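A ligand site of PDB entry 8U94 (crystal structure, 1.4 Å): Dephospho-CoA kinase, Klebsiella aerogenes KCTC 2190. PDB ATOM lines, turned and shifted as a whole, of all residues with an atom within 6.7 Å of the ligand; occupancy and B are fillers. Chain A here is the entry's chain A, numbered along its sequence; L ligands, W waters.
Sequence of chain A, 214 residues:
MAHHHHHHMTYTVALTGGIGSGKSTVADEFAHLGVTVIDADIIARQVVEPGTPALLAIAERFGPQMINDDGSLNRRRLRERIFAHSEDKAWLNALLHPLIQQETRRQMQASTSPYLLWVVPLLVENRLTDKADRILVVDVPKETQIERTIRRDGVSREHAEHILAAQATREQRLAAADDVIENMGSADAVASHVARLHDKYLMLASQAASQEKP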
ATOM      1  N   GLY A  17      19.173 -21.055 -27.478  1.00  0.00           N
ATOM      2  CA  GLY A  17      18.168 -20.752 -26.509  1.00  0.00           C
ATOM      3  C   GLY A  17      18.825 -20.604 -25.148  1.00  0.00           C
ATOM      4  O   GLY A  17      19.900 -21.166 -24.911  1.00  0.00           O
ATOM      5  N   GLY A  18      18.203 -19.862 -24.267  1.00  0.00           N
ATOM      6  CA  GLY A  18      18.712 -19.664 -22.932  1.00  0.00           C
ATOM      7  C   GLY A  18      18.603 -20.908 -22.087  1.00  0.00           C
ATOM      8  O   GLY A  18      17.953 -21.886 -22.436  1.00  0.00           O
ATOM      9  N   ILE A  19      19.226 -20.856 -20.919  1.00  0.00           N
ATOM     10  CA  ILE A  19      19.182 -22.004 -20.026  1.00  0.00           C
ATOM     11  C   ILE A  19      17.730 -22.338 -19.686  1.00  0.00           C
ATOM     12  O   ILE A  19      16.906 -21.453 -19.421  1.00  0.00           O
ATOM     13  CB  ILE A  19      20.006 -21.740 -18.753  1.00  0.00           C
ATOM     14  CG1 ILE A  19      20.111 -23.005 -17.895  1.00  0.00           C
ATOM     15  CG2 ILE A  19      19.426 -20.568 -17.951  1.00  0.00           C
ATOM     16  CD1 ILE A  19      21.103 -22.948 -16.745  1.00  0.00           C
ATOM     17  N   GLY A  20      17.408 -23.617 -19.730  1.00  0.00           N
ATOM     18  CA  GLY A  20      16.099 -24.074 -19.356  1.00  0.00           C
ATOM     19  C   GLY A  20      15.018 -23.854 -20.402  1.00  0.00           C
ATOM     20  O   GLY A  20      13.866 -24.178 -20.131  1.00  0.00           O
ATOM     21  N   SER A  21      15.357 -23.353 -21.581  1.00  0.00           N
ATOM     22  CA  SER A  21      14.324 -23.061 -22.576  1.00  0.00           C
ATOM     23  C   SER A  21      13.866 -24.308 -23.313  1.00  0.00           C
ATOM     24  O   SER A  21      12.726 -24.341 -23.775  1.00  0.00           O
ATOM     25  CB  SER A  21      14.848 -22.020 -23.566  1.00  0.00           C
ATOM     26  OG  SER A  21      16.008 -22.481 -24.258  1.00  0.00           O
ATOM     27  N   GLY A  22      14.734 -25.305 -23.459  1.00  0.00           N
ATOM     28  CA  GLY A  22      14.355 -26.557 -24.092  1.00  0.00           C
ATOM     29  C   GLY A  22      15.201 -26.941 -25.287  1.00  0.00           C
ATOM     30  O   GLY A  22      14.722 -27.640 -26.185  1.00  0.00           O
ATOM     31  N   LYS A  23      16.461 -26.516 -25.329  1.00  0.00           N
ATOM     32  CA  LYS A  23      17.333 -26.921 -26.419  1.00  0.00           C
ATOM     33  C   LYS A  23      17.411 -28.449 -26.520  1.00  0.00           C
ATOM     34  O   LYS A  23      17.205 -29.022 -27.599  1.00  0.00           O
ATOM     35  CB  LYS A  23      18.729 -26.326 -26.215  1.00  0.00           C
ATOM     36  CG  LYS A  23      18.804 -24.815 -26.417  1.00  0.00           C
ATOM     37  CD  LYS A  23      20.200 -24.258 -26.215  1.00  0.00           C
ATOM     38  CE  LYS A  23      20.697 -24.434 -24.803  1.00  0.00           C
ATOM     39  NZ  LYS A  23      19.814 -23.765 -23.776  1.00  0.00           N
ATOM     40  N   SER A  24      17.741 -29.124 -25.414  1.00  0.00           N
ATOM     41  CA  SER A  24      17.836 -30.581 -25.446  1.00  0.00           C
ATOM     42  C   SER A  24      16.494 -31.210 -25.826  1.00  0.00           C
ATOM     43  O   SER A  24      16.449 -32.194 -26.584  1.00  0.00           O
ATOM     44  CB  SER A  24      18.287 -31.106 -24.073  1.00  0.00           C
ATOM     45  OG  SER A  24      19.587 -30.665 -23.740  1.00  0.00           O
ATOM     46  N   THR A  25      15.405 -30.644 -25.331  1.00  0.00           N
ATOM     47  CA  THR A  25      14.080 -31.229 -25.573  1.00  0.00           C
ATOM     48  C   THR A  25      13.691 -31.139 -27.046  1.00  0.00           C
ATOM     49  O   THR A  25      13.233 -32.123 -27.642  1.00  0.00           O
ATOM     50  CB  THR A  25      13.087 -30.458 -24.688  1.00  0.00           C
ATOM     51  OG1 THR A  25      13.468 -30.579 -23.302  1.00  0.00           O
ATOM     52  CG2 THR A  25      11.716 -30.995 -24.882  1.00  0.00           C
ATOM     53  N   VAL A  26      13.857 -29.973 -27.643  1.00  0.00           N
ATOM     54  CA  VAL A  26      13.554 -29.790 -29.065  1.00  0.00           C
ATOM     55  C   VAL A  26      14.519 -30.593 -29.942  1.00  0.00           C
ATOM     56  O   VAL A  26      14.089 -31.202 -30.926  1.00  0.00           O
ATOM     57  CB  VAL A  26      13.562 -28.284 -29.364  1.00  0.00           C
ATOM     58  CG1 VAL A  26      13.594 -28.024 -30.847  1.00  0.00           C
ATOM     59  CG2 VAL A  26      12.348 -27.631 -28.696  1.00  0.00           C
ATOM     60  N   ASP A  39      25.814 -32.285 -30.309  1.00  0.00           N
ATOM     61  CA  ASP A  39      25.713 -31.531 -29.061  1.00  0.00           C
ATOM     62  C   ASP A  39      26.973 -31.789 -28.238  1.00  0.00           C
ATOM     63  O   ASP A  39      27.205 -32.902 -27.756  1.00  0.00           O
ATOM     64  CB  ASP A  39      24.449 -31.942 -28.313  1.00  0.00           C
ATOM     65  CG  ASP A  39      24.213 -31.127 -27.054  1.00  0.00           C
ATOM     66  OD1 ASP A  39      25.166 -30.534 -26.494  1.00  0.00           O
ATOM     67  OD2 ASP A  39      23.050 -31.103 -26.620  1.00  0.00           O
ATOM     68  N   VAL A 119      23.494 -28.125 -31.638  1.00  0.00           N
ATOM     69  CA  VAL A 119      23.053 -27.466 -30.431  1.00  0.00           C
ATOM     70  C   VAL A 119      24.182 -26.567 -29.944  1.00  0.00           C
ATOM     71  O   VAL A 119      25.266 -27.063 -29.592  1.00  0.00           O
ATOM     72  CB  VAL A 119      22.634 -28.486 -29.360  1.00  0.00           C
ATOM     73  CG1 VAL A 119      22.126 -27.788 -28.129  1.00  0.00           C
ATOM     74  CG2 VAL A 119      21.601 -29.478 -29.904  1.00  0.00           C
ATOM     75  N   VAL A 138      14.950 -21.653 -29.532  1.00  0.00           N
ATOM     76  CA  VAL A 138      13.914 -22.160 -28.633  1.00  0.00           C
ATOM     77  C   VAL A 138      13.669 -21.100 -27.576  1.00  0.00           C
ATOM     78  O   VAL A 138      14.595 -20.702 -26.863  1.00  0.00           O
ATOM     79  CB  VAL A 138      14.316 -23.511 -28.005  1.00  0.00           C
ATOM     80  CG1 VAL A 138      13.166 -24.117 -27.194  1.00  0.00           C
ATOM     81  CG2 VAL A 138      14.815 -24.477 -29.055  1.00  0.00           C
ATOM     82  N   THR A 144       9.461 -18.809 -17.113  1.00  0.00           N
ATOM     83  CA  THR A 144       9.518 -20.233 -17.409  1.00  0.00           C
ATOM     84  C   THR A 144      10.954 -20.747 -17.375  1.00  0.00           C
ATOM     85  O   THR A 144      11.204 -21.826 -16.825  1.00  0.00           O
ATOM     86  CB  THR A 144       8.871 -20.466 -18.766  1.00  0.00           C
ATOM     87  OG1 THR A 144       7.508 -19.983 -18.767  1.00  0.00           O
ATOM     88  CG2 THR A 144       8.916 -21.931 -19.133  1.00  0.00           C
ATOM     89  N   ARG A 148      11.982 -23.723 -14.769  1.00  0.00           N
ATOM     90  CA  ARG A 148      12.506 -24.993 -15.265  1.00  0.00           C
ATOM     91  C   ARG A 148      13.964 -25.221 -14.851  1.00  0.00           C
ATOM     92  O   ARG A 148      14.367 -26.367 -14.653  1.00  0.00           O
ATOM     93  CB  ARG A 148      12.348 -25.059 -16.782  1.00  0.00           C
ATOM     94  CG  ARG A 148      10.889 -25.073 -17.222  1.00  0.00           C
ATOM     95  CD  ARG A 148      10.731 -25.253 -18.721  1.00  0.00           C
ATOM     96  NE  ARG A 148       9.326 -25.142 -19.106  1.00  0.00           N
ATOM     97  CZ  ARG A 148       8.902 -25.034 -20.360  1.00  0.00           C
ATOM     98  NH1 ARG A 148       9.735 -25.151 -21.387  1.00  0.00           N
ATOM     99  NH2 ARG A 148       7.621 -24.787 -20.602  1.00  0.00           N
ATOM    100  N   THR A 149      14.735 -24.146 -14.705  1.00  0.00           N
ATOM    101  CA  THR A 149      16.120 -24.277 -14.263  1.00  0.00           C
ATOM    102  C   THR A 149      16.201 -24.615 -12.783  1.00  0.00           C
ATOM    103  O   THR A 149      16.997 -25.463 -12.383  1.00  0.00           O
ATOM    104  CB  THR A 149      16.877 -22.976 -14.549  1.00  0.00           C
ATOM    105  OG1 THR A 149      16.886 -22.728 -15.947  1.00  0.00           O
ATOM    106  CG2 THR A 149      18.317 -23.096 -14.010  1.00  0.00           C
ATOM    107  N   ARG A 151      14.060 -26.320 -11.116  1.00  0.00           N
ATOM    108  CA  ARG A 151      13.638 -27.703 -10.946  1.00  0.00           C
ATOM    109  C   ARG A 151      14.695 -28.681 -11.447  1.00  0.00           C
ATOM    110  O   ARG A 151      14.961 -29.696 -10.796  1.00  0.00           O
ATOM    111  CB  ARG A 151      12.333 -27.936 -11.697  1.00  0.00           C
ATOM    112  CG  ARG A 151      11.117 -27.326 -11.023  1.00  0.00           C
ATOM    113  CD  ARG A 151       9.861 -27.942 -11.626  1.00  0.00           C
ATOM    114  NE  ARG A 151       8.944 -26.945 -12.149  1.00  0.00           N
ATOM    115  CZ  ARG A 151       7.806 -26.581 -11.574  1.00  0.00           C
ATOM    116  NH1 ARG A 151       7.403 -27.124 -10.428  1.00  0.00           N
ATOM    117  NH2 ARG A 151       7.042 -25.669 -12.160  1.00  0.00           N
ATOM    118  N   ARG A 152      15.275 -28.411 -12.622  1.00  0.00           N
ATOM    119  CA  ARG A 152      16.235 -29.339 -13.187  1.00  0.00           C
ATOM    120  C   ARG A 152      17.548 -29.311 -12.407  1.00  0.00           C
ATOM    121  O   ARG A 152      18.146 -30.363 -12.168  1.00  0.00           O
ATOM    122  CB  ARG A 152      16.508 -28.997 -14.652  1.00  0.00           C
ATOM    123  CG  ARG A 152      17.352 -30.059 -15.357  1.00  0.00           C
ATOM    124  CD  ARG A 152      17.831 -29.581 -16.734  1.00  0.00           C
ATOM    125  NE  ARG A 152      18.724 -28.450 -16.592  1.00  0.00           N
ATOM    126  CZ  ARG A 152      19.044 -27.595 -17.542  1.00  0.00           C
ATOM    127  NH1 ARG A 152      18.551 -27.711 -18.762  1.00  0.00           N
ATOM    128  NH2 ARG A 152      19.868 -26.591 -17.270  1.00  0.00           N
ATOM    129  N   ASP A 153      18.020 -28.135 -12.034  1.00  0.00           N
ATOM    130  CA  ASP A 153      19.383 -27.971 -11.547  1.00  0.00           C
ATOM    131  C   ASP A 153      19.486 -27.756 -10.048  1.00  0.00           C
ATOM    132  O   ASP A 153      20.605 -27.742  -9.530  1.00  0.00           O
ATOM    133  CB  ASP A 153      20.059 -26.797 -12.276  1.00  0.00           C
ATOM    134  CG  ASP A 153      20.328 -27.098 -13.744  1.00  0.00           C
ATOM    135  OD1 ASP A 153      20.198 -28.277 -14.147  1.00  0.00           O
ATOM    136  OD2 ASP A 153      20.671 -26.156 -14.473  1.00  0.00           O
ATOM    137  N   ASN A 183       8.686 -23.285 -26.734  1.00  0.00           N
ATOM    138  CA  ASN A 183       8.561 -24.601 -26.086  1.00  0.00           C
ATOM    139  C   ASN A 183       7.564 -24.466 -24.934  1.00  0.00           C
ATOM    140  O   ASN A 183       7.902 -24.572 -23.763  1.00  0.00           O
ATOM    141  CB  ASN A 183       9.923 -25.105 -25.620  1.00  0.00           C
ATOM    142  CG  ASN A 183       9.832 -26.447 -24.981  1.00  0.00           C
ATOM    143  OD1 ASN A 183       8.935 -27.251 -25.265  1.00  0.00           O
ATOM    144  ND2 ASN A 183      10.783 -26.718 -24.094  1.00  0.00           N
ATOM    145  N   MET A 184       6.305 -24.240 -25.337  1.00  0.00           N
ATOM    146  CA  MET A 184       5.211 -23.922 -24.430  1.00  0.00           C
ATOM    147  C   MET A 184       3.956 -24.578 -24.986  1.00  0.00           C
ATOM    148  O   MET A 184       3.895 -24.937 -26.162  1.00  0.00           O
ATOM    149  CB  MET A 184       4.978 -22.416 -24.347  1.00  0.00           C
ATOM    150  CG  MET A 184       6.189 -21.650 -23.886  1.00  0.00           C
ATOM    151  SD  MET A 184       6.646 -21.942 -22.164  1.00  0.00           S
ATOM    152  CE  MET A 184       5.316 -21.093 -21.307  1.00  0.00           C
ATOM    153  N   GLY A 185       2.957 -24.729 -24.132  1.00  0.00           N
ATOM    154  CA  GLY A 185       1.739 -25.369 -24.553  1.00  0.00           C
ATOM    155  C   GLY A 185       1.881 -26.876 -24.610  1.00  0.00           C
ATOM    156  O   GLY A 185       2.742 -27.487 -23.968  1.00  0.00           O
ATOM    157  N   SER A 186       1.015 -27.489 -25.402  1.00  0.00           N
ATOM    158  CA  SER A 186       0.972 -28.943 -25.479  1.00  0.00           C
ATOM    159  C   SER A 186       2.222 -29.485 -26.170  1.00  0.00           C
ATOM    160  O   SER A 186       2.705 -28.914 -27.161  1.00  0.00           O
ATOM    161  CB  SER A 186      -0.271 -29.395 -26.236  1.00  0.00           C
ATOM    162  OG  SER A 186      -0.064 -29.298 -27.631  1.00  0.00           O
ATOM    163  N   ALA A 187       2.739 -30.599 -25.642  1.00  0.00           N
ATOM    164  CA  ALA A 187       3.933 -31.198 -26.224  1.00  0.00           C
ATOM    165  C   ALA A 187       3.679 -31.697 -27.640  1.00  0.00           C
ATOM    166  O   ALA A 187       4.577 -31.642 -28.488  1.00  0.00           O
ATOM    167  CB  ALA A 187       4.428 -32.355 -25.342  1.00  0.00           C
ATOM    168  N   VAL A 190       4.171 -28.732 -29.923  1.00  0.00           N
ATOM    169  CA  VAL A 190       5.592 -28.455 -30.110  1.00  0.00           C
ATOM    170  C   VAL A 190       6.199 -29.443 -31.111  1.00  0.00           C
ATOM    171  O   VAL A 190       6.958 -29.053 -32.001  1.00  0.00           O
ATOM    172  CB  VAL A 190       6.341 -28.438 -28.771  1.00  0.00           C
ATOM    173  CG1 VAL A 190       7.850 -28.278 -28.983  1.00  0.00           C
ATOM    174  CG2 VAL A 190       5.814 -27.316 -27.879  1.00  0.00           C
HETATM  175  P1  LIG L   1      18.044 -26.457 -22.183  1.00  0.00           P
HETATM  176  O1  LIG L   1      18.790 -25.953 -20.931  1.00  0.00           O
HETATM  177  O2  LIG L   1      18.710 -27.631 -22.926  1.00  0.00           O
HETATM  178  O3  LIG L   1      17.684 -25.360 -23.100  1.00  0.00           O
HETATM  179  P2  LIG L   1      16.110 -28.528 -21.479  1.00  0.00           P
HETATM  180  O4  LIG L   1      17.087 -29.346 -20.643  1.00  0.00           O
HETATM  181  O5  LIG L   1      15.626 -29.073 -22.834  1.00  0.00           O
HETATM  182  O6  LIG L   1      16.622 -27.026 -21.616  1.00  0.00           O
HETATM  183  O7  LIG L   1      14.779 -28.261 -20.617  1.00  0.00           O
HETATM  184  C1  LIG L   1      14.917 -27.676 -19.320  1.00  0.00           C
HETATM  185  C2  LIG L   1      14.005 -28.376 -18.328  1.00  0.00           C
HETATM  186  O8  LIG L   1      12.632 -28.210 -18.691  1.00  0.00           O
HETATM  187  C3  LIG L   1      14.245 -29.885 -18.273  1.00  0.00           C
HETATM  188  O9  LIG L   1      14.126 -30.285 -16.914  1.00  0.00           O
HETATM  189  C4  LIG L   1      13.124 -30.477 -19.115  1.00  0.00           C
HETATM  190  O10 LIG L   1      12.677 -31.761 -18.726  1.00  0.00           O
HETATM  191  C5  LIG L   1      11.997 -29.510 -18.853  1.00  0.00           C
HETATM  192  N1  LIG L   1      11.053 -29.252 -19.926  1.00  0.00           N
HETATM  193  C6  LIG L   1      11.318 -29.283 -21.248  1.00  0.00           C
HETATM  194  N2  LIG L   1      10.220 -28.946 -21.947  1.00  0.00           N
HETATM  195  C7  LIG L   1       9.259 -28.659 -21.042  1.00  0.00           C
HETATM  196  C8  LIG L   1       7.864 -28.230 -21.090  1.00  0.00           C
HETATM  197  N3  LIG L   1       7.312 -28.028 -22.295  1.00  0.00           N
HETATM  198  N4  LIG L   1       7.213 -28.057 -19.925  1.00  0.00           N
HETATM  199  C9  LIG L   1       7.799 -28.248 -18.729  1.00  0.00           C
HETATM  200  N5  LIG L   1       9.074 -28.643 -18.610  1.00  0.00           N
HETATM  201  C10 LIG L   1       9.812 -28.854 -19.718  1.00  0.00           C
HETATM  202  O   HOH W   1       8.198 -31.512 -23.183  1.00  0.00           O
HETATM  203  O   HOH W   2      21.281 -26.132 -20.007  1.00  0.00           O
HETATM  204  O   HOH W   3       5.251 -29.207 -24.081  1.00  0.00           O
HETATM  205  O   HOH W   4      12.650 -28.567 -15.279  1.00  0.00           O
HETATM  206  O   HOH W   5       9.867 -28.530 -15.799  1.00  0.00           O
HETATM  207  O   HOH W   6      21.572 -24.219 -21.808  1.00  0.00           O
HETATM  208  O   HOH W   7      16.942 -32.018 -20.235  1.00  0.00           O
HETATM  209  O   HOH W   8      19.827 -30.015 -21.104  1.00  0.00           O
HETATM  210  O   HOH W   9      12.357 -26.225 -21.340  1.00  0.00           O
HETATM  211  O   HOH W  10       7.568 -29.616 -25.190  1.00  0.00           O
HETATM  212  O   HOH W  11      14.788 -32.881 -16.462  1.00  0.00           O
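N of Thr 25 is in hydrogen-bond range of O5 of the ligand (3.0 Å).
The side-chain hydroxyl of Thr 25 lies within hydrogen-bond range of an oxygen (O5) of the ligand (2.7 Å).
The backbone NH of Lys 23 lies within hydrogen-bond range of an oxygen (O3) of the ligand, at 2.8 Å.
O3 of the ligand is in salt-bridge range of NZ of Lys 23 (2.7 Å).
The guanidinium group (NH1) of Arg 152 is in salt-bridge range of an oxygen (O1) of the ligand.
O1 of the ligand sits at hydrogen-bond distance from N of Gly 20 (3.0 Å).
An oxygen (O3) of the ligand sits at hydrogen-bond distance from the backbone NH (N) of Gly 22, 3.0 Å away.
An oxygen (O2) of the ligand lies within hydrogen-bond range of the backbone NH (N) of Ser 24 (3.1 Å).
The side-chain hydroxyl (OG) of Ser 24 is in hydrogen-bond range of an oxygen (O2) of the ligand (3.3 Å).
A nitrogen (N2) of the ligand lies within hydrogen-bond range of the side-chain amide nitrogen (ND2) of Asn 183 (3.1 Å).
NH2 of Arg 148 lies within hydrogen-bond range of N4 of the ligand (3.4 Å).
O3 of the ligand is in hydrogen-bond range of N of Ser 21 (3.4 Å).
O of Gly 18 sits at hydrogen-bond distance from NZ of Lys 23, at 3.0 Å.
The side-chain amino group (NZ) of Lys 23 lies within hydrogen-bond range of the backbone carbonyl oxygen (O) of Gly 17 (2.8 Å).
The side-chain carboxylate (OD1) of Asp 153 is in salt-bridge range of the guanidinium group (NE) of Arg 152, at 2.9 Å.
NH1 of Arg 148 sits at hydrogen-bond distance from O of Asn 183, 3.1 Å away.
The side-chain amide nitrogen of Asn 183 lies within hydrogen-bond range of the backbone carbonyl oxygen of Ser 21, at 3.1 Å.
The guanidinium group (NH2) of Arg 148 is in hydrogen-bond range of the side-chain sulfur (SD) of Met 184, 3.4 Å away.
O of Gly 18 lies within hydrogen-bond range of OG of Ser 21 (2.7 Å).
The side-chain hydroxyl (OG) of Ser 21 lies within hydrogen-bond range of the backbone carbonyl oxygen (O) of Val 138, at 3.5 Å.
Gly 18 touches the ligand (O to O3, 3.5 Å).
Ile 19 touches the ligand.
11 residues have an atom within 4 Å of the ligand: Gly 18, Ile 19, Gly 20, Ser 21, Gly 22, Lys 23, Ser 24, Thr 25, Arg 148, Arg 152 and Asn 183.
Water W2 lies within hydrogen-bond range of O1 of the ligand (2.7 Å) and NH2 of Arg 152 (3.1 Å).
Water W4 bridges an oxygen (O9) of the ligand (2.8 Å) and the backbone carbonyl oxygen of Arg 148 (2.9 Å).
Water W8 lies within hydrogen-bond range of the side-chain hydroxyl (OG) of Ser 24 and an oxygen (O4) of the ligand.
Water W3 lies within hydrogen-bond range of a nitrogen (N3) of the ligand, the backbone carbonyl oxygen (O) of Gly 185 and the backbone NH (N) of Ala 187.
Water W10 bridges the side-chain amide oxygen of Asn 183 (2.7 Å) and a nitrogen (N3) of the ligand (3.3 Å).
Water W6 bridges NZ of Lys 23 and O1 of the ligand.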
